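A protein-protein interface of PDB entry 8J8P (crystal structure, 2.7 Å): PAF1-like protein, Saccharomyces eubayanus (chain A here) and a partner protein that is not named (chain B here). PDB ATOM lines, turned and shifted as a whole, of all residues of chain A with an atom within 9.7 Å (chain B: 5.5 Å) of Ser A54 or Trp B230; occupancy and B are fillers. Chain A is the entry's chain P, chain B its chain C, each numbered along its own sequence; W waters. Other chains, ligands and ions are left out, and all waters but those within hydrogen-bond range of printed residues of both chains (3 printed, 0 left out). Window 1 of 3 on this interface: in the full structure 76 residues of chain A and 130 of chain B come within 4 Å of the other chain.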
ATOM      1  N   LEU A  47     -16.731  -7.235  31.098  1.00  0.00           N
ATOM      2  CA  LEU A  47     -16.424  -5.896  30.602  1.00  0.00           C
ATOM      3  C   LEU A  47     -15.212  -5.307  31.325  1.00  0.00           C
ATOM      4  O   LEU A  47     -14.368  -4.637  30.705  1.00  0.00           O
ATOM      5  CB  LEU A  47     -17.647  -4.985  30.741  1.00  0.00           C
ATOM      6  CG  LEU A  47     -17.499  -3.542  30.251  1.00  0.00           C
ATOM      7  CD1 LEU A  47     -16.915  -3.481  28.843  1.00  0.00           C
ATOM      8  CD2 LEU A  47     -18.835  -2.829  30.292  1.00  0.00           C
ATOM      9  N   TYR A  48     -15.103  -5.559  32.635  1.00  0.00           N
ATOM     10  CA  TYR A  48     -13.968  -5.047  33.398  1.00  0.00           C
ATOM     11  C   TYR A  48     -12.661  -5.506  32.791  1.00  0.00           C
ATOM     12  O   TYR A  48     -11.671  -4.769  32.802  1.00  0.00           O
ATOM     13  CB  TYR A  48     -14.026  -5.512  34.853  1.00  0.00           C
ATOM     14  CG  TYR A  48     -12.843  -4.991  35.634  1.00  0.00           C
ATOM     15  CD1 TYR A  48     -11.695  -5.765  35.821  1.00  0.00           C
ATOM     16  CD2 TYR A  48     -12.857  -3.701  36.154  1.00  0.00           C
ATOM     17  CE1 TYR A  48     -10.594  -5.262  36.525  1.00  0.00           C
ATOM     18  CE2 TYR A  48     -11.776  -3.194  36.850  1.00  0.00           C
ATOM     19  CZ  TYR A  48     -10.647  -3.972  37.035  1.00  0.00           C
ATOM     20  OH  TYR A  48      -9.584  -3.435  37.736  1.00  0.00           O
ATOM     21  N   VAL A  49     -12.630  -6.747  32.301  1.00  0.00           N
ATOM     22  CA  VAL A  49     -11.416  -7.254  31.662  1.00  0.00           C
ATOM     23  C   VAL A  49     -10.960  -6.298  30.567  1.00  0.00           C
ATOM     24  O   VAL A  49      -9.770  -5.966  30.461  1.00  0.00           O
ATOM     25  CB  VAL A  49     -11.638  -8.678  31.114  1.00  0.00           C
ATOM     26  CG1 VAL A  49     -10.506  -9.057  30.163  1.00  0.00           C
ATOM     27  CG2 VAL A  49     -11.730  -9.686  32.252  1.00  0.00           C
ATOM     28  N   LYS A  50     -11.903  -5.798  29.769  1.00  0.00           N
ATOM     29  CA  LYS A  50     -11.539  -4.960  28.630  1.00  0.00           C
ATOM     30  C   LYS A  50     -11.247  -3.523  29.053  1.00  0.00           C
ATOM     31  O   LYS A  50     -10.258  -2.928  28.612  1.00  0.00           O
ATOM     32  CB  LYS A  50     -12.653  -5.006  27.581  1.00  0.00           C
ATOM     33  CG  LYS A  50     -13.215  -6.399  27.369  1.00  0.00           C
ATOM     34  CD  LYS A  50     -14.066  -6.477  26.110  1.00  0.00           C
ATOM     35  CE  LYS A  50     -15.553  -6.411  26.434  1.00  0.00           C
ATOM     36  NZ  LYS A  50     -16.325  -5.690  25.376  1.00  0.00           N
ATOM     37  N   THR A  51     -12.089  -2.945  29.903  1.00  0.00           N
ATOM     38  CA  THR A  51     -11.883  -1.590  30.421  1.00  0.00           C
ATOM     39  C   THR A  51     -11.739  -1.713  31.930  1.00  0.00           C
ATOM     40  O   THR A  51     -12.739  -1.823  32.650  1.00  0.00           O
ATOM     41  CB  THR A  51     -13.044  -0.673  30.067  1.00  0.00           C
ATOM     42  OG1 THR A  51     -14.162  -1.001  30.903  1.00  0.00           O
ATOM     43  CG2 THR A  51     -13.437  -0.864  28.609  1.00  0.00           C
ATOM     44  N   ASN A  52     -10.505  -1.691  32.417  1.00  0.00           N
ATOM     45  CA  ASN A  52     -10.258  -2.078  33.799  1.00  0.00           C
ATOM     46  C   ASN A  52      -9.996  -0.861  34.672  1.00  0.00           C
ATOM     47  O   ASN A  52     -10.907  -0.365  35.342  1.00  0.00           O
ATOM     48  CB  ASN A  52      -9.087  -3.056  33.843  1.00  0.00           C
ATOM     49  CG  ASN A  52      -8.029  -2.723  32.811  1.00  0.00           C
ATOM     50  OD1 ASN A  52      -7.344  -1.701  32.905  1.00  0.00           O
ATOM     51  ND2 ASN A  52      -7.945  -3.549  31.771  1.00  0.00           N
ATOM     52  N   ILE A  53      -8.758  -0.369  34.666  1.00  0.00           N
ATOM     53  CA  ILE A  53      -8.360   0.737  35.523  1.00  0.00           C
ATOM     54  C   ILE A  53      -8.448   2.076  34.801  1.00  0.00           C
ATOM     55  O   ILE A  53      -7.937   3.086  35.303  1.00  0.00           O
ATOM     56  CB  ILE A  53      -6.949   0.499  36.080  1.00  0.00           C
ATOM     57  CG1 ILE A  53      -5.981   0.145  34.944  1.00  0.00           C
ATOM     58  CG2 ILE A  53      -6.988  -0.649  37.088  1.00  0.00           C
ATOM     59  CD1 ILE A  53      -5.408   1.348  34.182  1.00  0.00           C
ATOM     60  N   SER A  54      -9.086   2.108  33.628  1.00  0.00           N
ATOM     61  CA  SER A  54      -9.069   3.311  32.800  1.00  0.00           C
ATOM     62  C   SER A  54      -9.442   4.555  33.593  1.00  0.00           C
ATOM     63  O   SER A  54      -8.779   5.592  33.478  1.00  0.00           O
ATOM     64  CB  SER A  54     -10.007   3.145  31.607  1.00  0.00           C
ATOM     65  OG  SER A  54      -9.802   4.202  30.683  1.00  0.00           O
ATOM     66  N   ASN A  55     -10.480   4.476  34.422  1.00  0.00           N
ATOM     67  CA  ASN A  55     -10.939   5.668  35.133  1.00  0.00           C
ATOM     68  C   ASN A  55     -10.041   6.056  36.301  1.00  0.00           C
ATOM     69  O   ASN A  55     -10.411   6.950  37.063  1.00  0.00           O
ATOM     70  CB  ASN A  55     -12.372   5.471  35.633  1.00  0.00           C
ATOM     71  CG  ASN A  55     -13.397   5.551  34.516  1.00  0.00           C
ATOM     72  OD1 ASN A  55     -13.160   6.188  33.486  1.00  0.00           O
ATOM     73  ND2 ASN A  55     -14.539   4.887  34.706  1.00  0.00           N
ATOM     74  N   LEU A  56      -8.880   5.423  36.475  1.00  0.00           N
ATOM     75  CA  LEU A  56      -7.986   5.777  37.567  1.00  0.00           C
ATOM     76  C   LEU A  56      -6.711   6.472  37.110  1.00  0.00           C
ATOM     77  O   LEU A  56      -6.030   7.072  37.950  1.00  0.00           O
ATOM     78  CB  LEU A  56      -7.608   4.528  38.379  1.00  0.00           C
ATOM     79  CG  LEU A  56      -8.727   3.794  39.114  1.00  0.00           C
ATOM     80  CD1 LEU A  56      -8.240   2.429  39.566  1.00  0.00           C
ATOM     81  CD2 LEU A  56      -9.256   4.589  40.304  1.00  0.00           C
ATOM     82  N   ILE A  57      -6.384   6.430  35.807  1.00  0.00           N
ATOM     83  CA  ILE A  57      -5.095   6.929  35.324  1.00  0.00           C
ATOM     84  C   ILE A  57      -4.894   8.394  35.679  1.00  0.00           C
ATOM     85  O   ILE A  57      -3.758   8.839  35.869  1.00  0.00           O
ATOM     86  CB  ILE A  57      -4.961   6.699  33.811  1.00  0.00           C
ATOM     87  CG1 ILE A  57      -6.075   7.469  33.099  1.00  0.00           C
ATOM     88  CG2 ILE A  57      -5.049   5.211  33.494  1.00  0.00           C
ATOM     89  CD1 ILE A  57      -5.561   8.313  31.957  1.00  0.00           C
ATOM     90  N   GLN A  58      -5.969   9.151  35.826  1.00  0.00           N
ATOM     91  CA  GLN A  58      -5.864  10.494  36.383  1.00  0.00           C
ATOM     92  C   GLN A  58      -5.989  10.363  37.897  1.00  0.00           C
ATOM     93  O   GLN A  58      -7.062  10.053  38.422  1.00  0.00           O
ATOM     94  CB  GLN A  58      -6.931  11.420  35.811  1.00  0.00           C
ATOM     95  CG  GLN A  58      -7.075  12.692  36.606  1.00  0.00           C
ATOM     96  CD  GLN A  58      -8.365  13.448  36.273  1.00  0.00           C
ATOM     97  OE1 GLN A  58      -8.991  13.199  35.239  1.00  0.00           O
ATOM     98  NE2 GLN A  58      -8.752  14.391  37.142  1.00  0.00           N
ATOM     99  N   GLN A  59      -4.899  10.610  38.610  1.00  0.00           N
ATOM    100  CA  GLN A  59      -4.848  10.233  40.017  1.00  0.00           C
ATOM    101  C   GLN A  59      -5.466  11.295  40.913  1.00  0.00           C
ATOM    102  O   GLN A  59      -6.138  10.964  41.896  1.00  0.00           O
ATOM    103  CB  GLN A  59      -3.405   9.976  40.423  1.00  0.00           C
ATOM    104  CG  GLN A  59      -2.685   9.060  39.464  1.00  0.00           C
ATOM    105  CD  GLN A  59      -1.200   9.218  39.590  1.00  0.00           C
ATOM    106  OE1 GLN A  59      -0.646   9.087  40.689  1.00  0.00           O
ATOM    107  NE2 GLN A  59      -0.532   9.499  38.474  1.00  0.00           N
ATOM    108  N   PRO A 103      -1.087  10.152  18.319  1.00  0.00           N
ATOM    109  CA  PRO A 103      -1.774   9.002  18.916  1.00  0.00           C
ATOM    110  C   PRO A 103      -2.469   8.141  17.875  1.00  0.00           C
ATOM    111  O   PRO A 103      -2.770   8.581  16.761  1.00  0.00           O
ATOM    112  CB  PRO A 103      -2.788   9.646  19.867  1.00  0.00           C
ATOM    113  CG  PRO A 103      -2.986  11.026  19.336  1.00  0.00           C
ATOM    114  CD  PRO A 103      -1.676  11.435  18.742  1.00  0.00           C
ATOM    115  N   ARG A 104      -2.578   6.888  18.211  1.00  0.00           N
ATOM    116  CA  ARG A 104      -3.338   5.954  17.450  1.00  0.00           C
ATOM    117  C   ARG A 104      -2.950   5.965  16.051  1.00  0.00           C
ATOM    118  O   ARG A 104      -3.724   6.068  15.176  1.00  0.00           O
ATOM    119  CB  ARG A 104      -4.768   6.361  17.571  1.00  0.00           C
ATOM    120  CG  ARG A 104      -5.689   5.432  16.916  1.00  0.00           C
ATOM    121  CD  ARG A 104      -6.616   4.915  17.934  1.00  0.00           C
ATOM    122  NE  ARG A 104      -6.312   3.535  18.141  1.00  0.00           N
ATOM    123  CZ  ARG A 104      -7.208   2.707  18.609  1.00  0.00           C
ATOM    124  NH1 ARG A 104      -8.397   3.198  18.863  1.00  0.00           N
ATOM    125  NH2 ARG A 104      -6.926   1.427  18.820  1.00  0.00           N
ATOM    126  N   ILE B 225       2.040  13.414  28.753  1.00  0.00           N
ATOM    127  CA  ILE B 225       2.036  12.758  27.453  1.00  0.00           C
ATOM    128  C   ILE B 225       1.243  11.471  27.533  1.00  0.00           C
ATOM    129  O   ILE B 225       0.330  11.228  26.731  1.00  0.00           O
ATOM    130  CB  ILE B 225       3.475  12.496  26.978  1.00  0.00           C
ATOM    131  CG1 ILE B 225       4.183  13.811  26.679  1.00  0.00           C
ATOM    132  CG2 ILE B 225       3.467  11.597  25.756  1.00  0.00           C
ATOM    133  CD1 ILE B 225       5.629  13.628  26.217  1.00  0.00           C
ATOM    134  N   GLY B 226       1.581  10.623  28.509  1.00  0.00           N
ATOM    135  CA  GLY B 226       0.850   9.383  28.673  1.00  0.00           C
ATOM    136  C   GLY B 226      -0.624   9.614  28.938  1.00  0.00           C
ATOM    137  O   GLY B 226      -1.479   8.887  28.421  1.00  0.00           O
ATOM    138  N   LEU B 227      -0.948  10.623  29.752  1.00  0.00           N
ATOM    139  CA  LEU B 227      -2.355  10.889  30.045  1.00  0.00           C
ATOM    140  C   LEU B 227      -3.122  11.193  28.763  1.00  0.00           C
ATOM    141  O   LEU B 227      -4.194  10.632  28.515  1.00  0.00           O
ATOM    142  CB  LEU B 227      -2.481  12.042  31.043  1.00  0.00           C
ATOM    143  CG  LEU B 227      -2.063  11.756  32.492  1.00  0.00           C
ATOM    144  CD1 LEU B 227      -2.034  13.037  33.348  1.00  0.00           C
ATOM    145  CD2 LEU B 227      -2.992  10.743  33.100  1.00  0.00           C
ATOM    146  N   CYS B 228      -2.569  12.062  27.914  1.00  0.00           N
ATOM    147  CA  CYS B 228      -3.262  12.395  26.672  1.00  0.00           C
ATOM    148  C   CYS B 228      -3.337  11.201  25.733  1.00  0.00           C
ATOM    149  O   CYS B 228      -4.384  10.955  25.121  1.00  0.00           O
ATOM    150  CB  CYS B 228      -2.576  13.556  25.991  1.00  0.00           C
ATOM    151  SG  CYS B 228      -2.592  14.945  27.055  1.00  0.00           S
ATOM    152  N   PHE B 229      -2.234  10.451  25.597  1.00  0.00           N
ATOM    153  CA  PHE B 229      -2.258   9.226  24.800  1.00  0.00           C
ATOM    154  C   PHE B 229      -3.378   8.315  25.256  1.00  0.00           C
ATOM    155  O   PHE B 229      -4.096   7.726  24.435  1.00  0.00           O
ATOM    156  CB  PHE B 229      -0.919   8.496  24.913  1.00  0.00           C
ATOM    157  CG  PHE B 229       0.092   8.900  23.872  1.00  0.00           C
ATOM    158  CD1 PHE B 229      -0.274   9.011  22.537  1.00  0.00           C
ATOM    159  CD2 PHE B 229       1.412   9.158  24.227  1.00  0.00           C
ATOM    160  CE1 PHE B 229       0.655   9.373  21.573  1.00  0.00           C
ATOM    161  CE2 PHE B 229       2.348   9.517  23.271  1.00  0.00           C
ATOM    162  CZ  PHE B 229       1.971   9.626  21.942  1.00  0.00           C
ATOM    163  N   TRP B 230      -3.543   8.184  26.572  1.00  0.00           N
ATOM    164  CA  TRP B 230      -4.571   7.300  27.098  1.00  0.00           C
ATOM    165  C   TRP B 230      -5.959   7.816  26.758  1.00  0.00           C
ATOM    166  O   TRP B 230      -6.808   7.063  26.265  1.00  0.00           O
ATOM    167  CB  TRP B 230      -4.415   7.164  28.606  1.00  0.00           C
ATOM    168  CG  TRP B 230      -5.282   6.114  29.159  1.00  0.00           C
ATOM    169  CD1 TRP B 230      -6.599   6.223  29.476  1.00  0.00           C
ATOM    170  CD2 TRP B 230      -4.899   4.773  29.473  1.00  0.00           C
ATOM    171  NE1 TRP B 230      -7.065   5.025  29.966  1.00  0.00           N
ATOM    172  CE2 TRP B 230      -6.036   4.121  29.972  1.00  0.00           C
ATOM    173  CE3 TRP B 230      -3.699   4.064  29.386  1.00  0.00           C
ATOM    174  CZ2 TRP B 230      -6.014   2.798  30.384  1.00  0.00           C
ATOM    175  CZ3 TRP B 230      -3.680   2.746  29.795  1.00  0.00           C
ATOM    176  CH2 TRP B 230      -4.828   2.129  30.285  1.00  0.00           C
ATOM    177  N   GLN B 231      -6.220   9.097  27.033  1.00  0.00           N
ATOM    178  CA  GLN B 231      -7.553   9.622  26.749  1.00  0.00           C
ATOM    179  C   GLN B 231      -7.869   9.567  25.255  1.00  0.00           C
ATOM    180  O   GLN B 231      -9.035   9.428  24.873  1.00  0.00           O
ATOM    181  CB  GLN B 231      -7.678  11.047  27.280  1.00  0.00           C
ATOM    182  CG  GLN B 231      -7.561  11.151  28.803  1.00  0.00           C
ATOM    183  CD  GLN B 231      -8.578  10.273  29.517  1.00  0.00           C
ATOM    184  OE1 GLN B 231      -8.224   9.440  30.359  1.00  0.00           O
ATOM    185  NE2 GLN B 231      -9.851  10.446  29.172  1.00  0.00           N
ATOM    186  N   LEU B 232      -6.850   9.661  24.399  1.00  0.00           N
ATOM    187  CA  LEU B 232      -7.019   9.538  22.957  1.00  0.00           C
ATOM    188  C   LEU B 232      -7.003   8.089  22.487  1.00  0.00           C
ATOM    189  O   LEU B 232      -6.758   7.836  21.300  1.00  0.00           O
ATOM    190  CB  LEU B 232      -5.941  10.336  22.233  1.00  0.00           C
ATOM    191  CG  LEU B 232      -6.064  11.835  22.491  1.00  0.00           C
ATOM    192  CD1 LEU B 232      -4.789  12.571  22.103  1.00  0.00           C
ATOM    193  CD2 LEU B 232      -7.256  12.378  21.725  1.00  0.00           C
ATOM    194  N   LYS B 233      -7.226   7.144  23.401  1.00  0.00           N
ATOM    195  CA  LYS B 233      -7.394   5.726  23.078  1.00  0.00           C
ATOM    196  C   LYS B 233      -6.126   5.100  22.493  1.00  0.00           C
ATOM    197  O   LYS B 233      -6.184   4.233  21.613  1.00  0.00           O
ATOM    198  CB  LYS B 233      -8.596   5.519  22.155  1.00  0.00           C
ATOM    199  CG  LYS B 233      -9.923   5.661  22.882  1.00  0.00           C
ATOM    200  CD  LYS B 233     -11.072   5.981  21.939  1.00  0.00           C
ATOM    201  CE  LYS B 233     -12.398   5.912  22.679  1.00  0.00           C
ATOM    202  NZ  LYS B 233     -12.299   6.560  24.022  1.00  0.00           N
ATOM    203  N   ASP B 234      -4.967   5.495  23.023  1.00  0.00           N
ATOM    204  CA  ASP B 234      -3.683   4.886  22.674  1.00  0.00           C
ATOM    205  C   ASP B 234      -2.989   4.404  23.946  1.00  0.00           C
ATOM    206  O   ASP B 234      -1.984   4.981  24.379  1.00  0.00           O
ATOM    207  CB  ASP B 234      -2.801   5.874  21.913  1.00  0.00           C
ATOM    208  CG  ASP B 234      -1.641   5.195  21.200  1.00  0.00           C
ATOM    209  OD1 ASP B 234      -1.296   4.051  21.575  1.00  0.00           O
ATOM    210  OD2 ASP B 234      -1.072   5.812  20.263  1.00  0.00           O
ATOM    211  N   PRO B 235      -3.495   3.339  24.565  1.00  0.00           N
ATOM    212  CA  PRO B 235      -2.914   2.901  25.849  1.00  0.00           C
ATOM    213  C   PRO B 235      -1.476   2.421  25.747  1.00  0.00           C
ATOM    214  O   PRO B 235      -0.712   2.586  26.711  1.00  0.00           O
ATOM    215  CB  PRO B 235      -3.849   1.768  26.290  1.00  0.00           C
ATOM    216  CG  PRO B 235      -4.448   1.255  25.012  1.00  0.00           C
ATOM    217  CD  PRO B 235      -4.605   2.474  24.130  1.00  0.00           C
ATOM    218  N   ALA B 238       0.706   5.466  25.858  1.00  0.00           N
ATOM    219  CA  ALA B 238       0.587   6.022  27.202  1.00  0.00           C
ATOM    220  C   ALA B 238       1.485   5.266  28.171  1.00  0.00           C
ATOM    221  O   ALA B 238       2.269   5.873  28.918  1.00  0.00           O
ATOM    222  CB  ALA B 238      -0.868   5.971  27.669  1.00  0.00           C
ATOM    223  N   ILE B 239       1.408   3.935  28.143  1.00  0.00           N
ATOM    224  CA  ILE B 239       2.199   3.132  29.067  1.00  0.00           C
ATOM    225  C   ILE B 239       3.686   3.256  28.751  1.00  0.00           C
ATOM    226  O   ILE B 239       4.519   3.295  29.663  1.00  0.00           O
ATOM    227  CB  ILE B 239       1.723   1.670  29.052  1.00  0.00           C
ATOM    228  CG1 ILE B 239       0.263   1.598  29.482  1.00  0.00           C
ATOM    229  CG2 ILE B 239       2.551   0.796  30.012  1.00  0.00           C
ATOM    230  CD1 ILE B 239      -0.312   0.198  29.408  1.00  0.00           C
ATOM    231  N   TRP B 242       4.720   6.451  30.494  1.00  0.00           N
ATOM    232  CA  TRP B 242       4.815   6.354  31.954  1.00  0.00           C
ATOM    233  C   TRP B 242       6.000   5.492  32.374  1.00  0.00           C
ATOM    234  O   TRP B 242       6.713   5.826  33.332  1.00  0.00           O
ATOM    235  CB  TRP B 242       3.516   5.799  32.537  1.00  0.00           C
ATOM    236  CG  TRP B 242       2.354   6.675  32.219  1.00  0.00           C
ATOM    237  CD1 TRP B 242       2.384   8.022  32.026  1.00  0.00           C
ATOM    238  CD2 TRP B 242       0.988   6.269  32.030  1.00  0.00           C
ATOM    239  NE1 TRP B 242       1.118   8.492  31.733  1.00  0.00           N
ATOM    240  CE2 TRP B 242       0.246   7.433  31.728  1.00  0.00           C
ATOM    241  CE3 TRP B 242       0.325   5.041  32.090  1.00  0.00           C
ATOM    242  CZ2 TRP B 242      -1.129   7.404  31.491  1.00  0.00           C
ATOM    243  CZ3 TRP B 242      -1.049   5.010  31.853  1.00  0.00           C
ATOM    244  CH2 TRP B 242      -1.756   6.190  31.553  1.00  0.00           C
ATOM    245  N   HIS B 265      -3.500  -3.410  33.434  1.00  0.00           N
ATOM    246  CA  HIS B 265      -4.136  -3.377  32.117  1.00  0.00           C
ATOM    247  C   HIS B 265      -3.514  -4.404  31.177  1.00  0.00           C
ATOM    248  O   HIS B 265      -4.224  -5.178  30.522  1.00  0.00           O
ATOM    249  CB  HIS B 265      -4.016  -1.969  31.542  1.00  0.00           C
ATOM    250  CG  HIS B 265      -4.378  -1.861  30.094  1.00  0.00           C
ATOM    251  ND1 HIS B 265      -5.680  -1.703  29.664  1.00  0.00           N
ATOM    252  CD2 HIS B 265      -3.607  -1.828  28.980  1.00  0.00           C
ATOM    253  CE1 HIS B 265      -5.699  -1.614  28.344  1.00  0.00           C
ATOM    254  NE2 HIS B 265      -4.454  -1.686  27.905  1.00  0.00           N
HETATM  255  O   HOH W   1      -8.030  -0.183  30.198  1.00  0.00           O
HETATM  256  O   HOH W   2       0.832   6.244  18.519  1.00  0.00           O
HETATM  257  O   HOH W   3      -8.112   1.351  21.848  1.00  0.00           O
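Among the printed residues, pairs that only touch across the chains: Asn A52 with His B265 (3.6 Å), Ile A57 with Leu B227 (3.4 Å), Ile A57 with Trp B230 (3.4 Å), Ile A57 with Gln B231 (3.3 Å), Ile A57 with Trp B242 (3.9 Å), Pro A103 with Phe B229 (3.6 Å), Pro A103 with Leu B232 (3.6 Å), Pro A103 with Asp B234 (3.5 Å) and Arg A104 with Lys B233 (3.5 Å).
The backbone carbonyl oxygen (O) of Phe B229 lies within hydrogen-bond range of the backbone NH (N) of Asp B234 (2.8 Å). ND2 of Asn A52 sits at hydrogen-bond distance from O of Val A49 (3.3 Å).
Of the 15 printed residues of chain A, 5 touch a printed residue of chain B. Printed residues of chain A that touch a printed residue of chain B: Asn A52, Ser A54, Ile A57, Pro A103 and Arg A104. Hydrophobic or aromatic side chains of chain A within 4 Å of the printed part of chain B: Ile A57 and Pro A103. Hydrophobic or aromatic side chains of chain B that line the printed part of chain A: Leu B227, Phe B229, Trp B230, Leu B232, Trp B242 and His B265. Along chain B the printed residues that touch a printed residue of chain A span positions 227 to 265. Among the printed residues, 11 pairs touch across the chains. Among the printed residues, no Asp or Glu carboxylate lies within 4 Å of a Lys or Arg side-chain nitrogen of the other chain.
Ser A54 touches just one residue of chain B: Trp B230 (2.9 Å). Asn A55 touches none of the printed residues of chain B. Printed residues of chain A within 4 Å of Trp B230: Ser A54 and Ile A57. Of chain A, only Ile A57 comes within 4 Å of Gln B231. Of the printed residues of chain A, Lys B233 touches Arg A104 (3.5 Å). Printed residues of chain A within 4 Å of Trp B242: Ile A57. The nearest residue of chain B that does not touch Ser A54 is Gln B231 (5.0 Å). The nearest printed residue of chain A that does not touch Trp B242 is Ile A53 (6.2 Å).
The indole nitrogen (NE1) of Trp B230 is in hydrogen-bond range of the side-chain hydroxyl (OG) of Ser A54 (2.9 Å). The side-chain carboxylate (OD2) of Asp B234 sits at hydrogen-bond distance from the backbone NH (N) of Arg A104, 2.8 Å away.
Water W2 bridges the side-chain carboxylate (OD2) of Asp B234 (2.6 Å) and the backbone NH (N) of Arg A104 (3.5 Å). Water W1 lies within hydrogen-bond range of ND1 of His B265 (2.8 Å) and OD1 of Asn A52 (3.2 Å). Water W3 bridges NH2 of Arg A104 (3.3 Å) and O of Lys B233 (3.5 Å).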
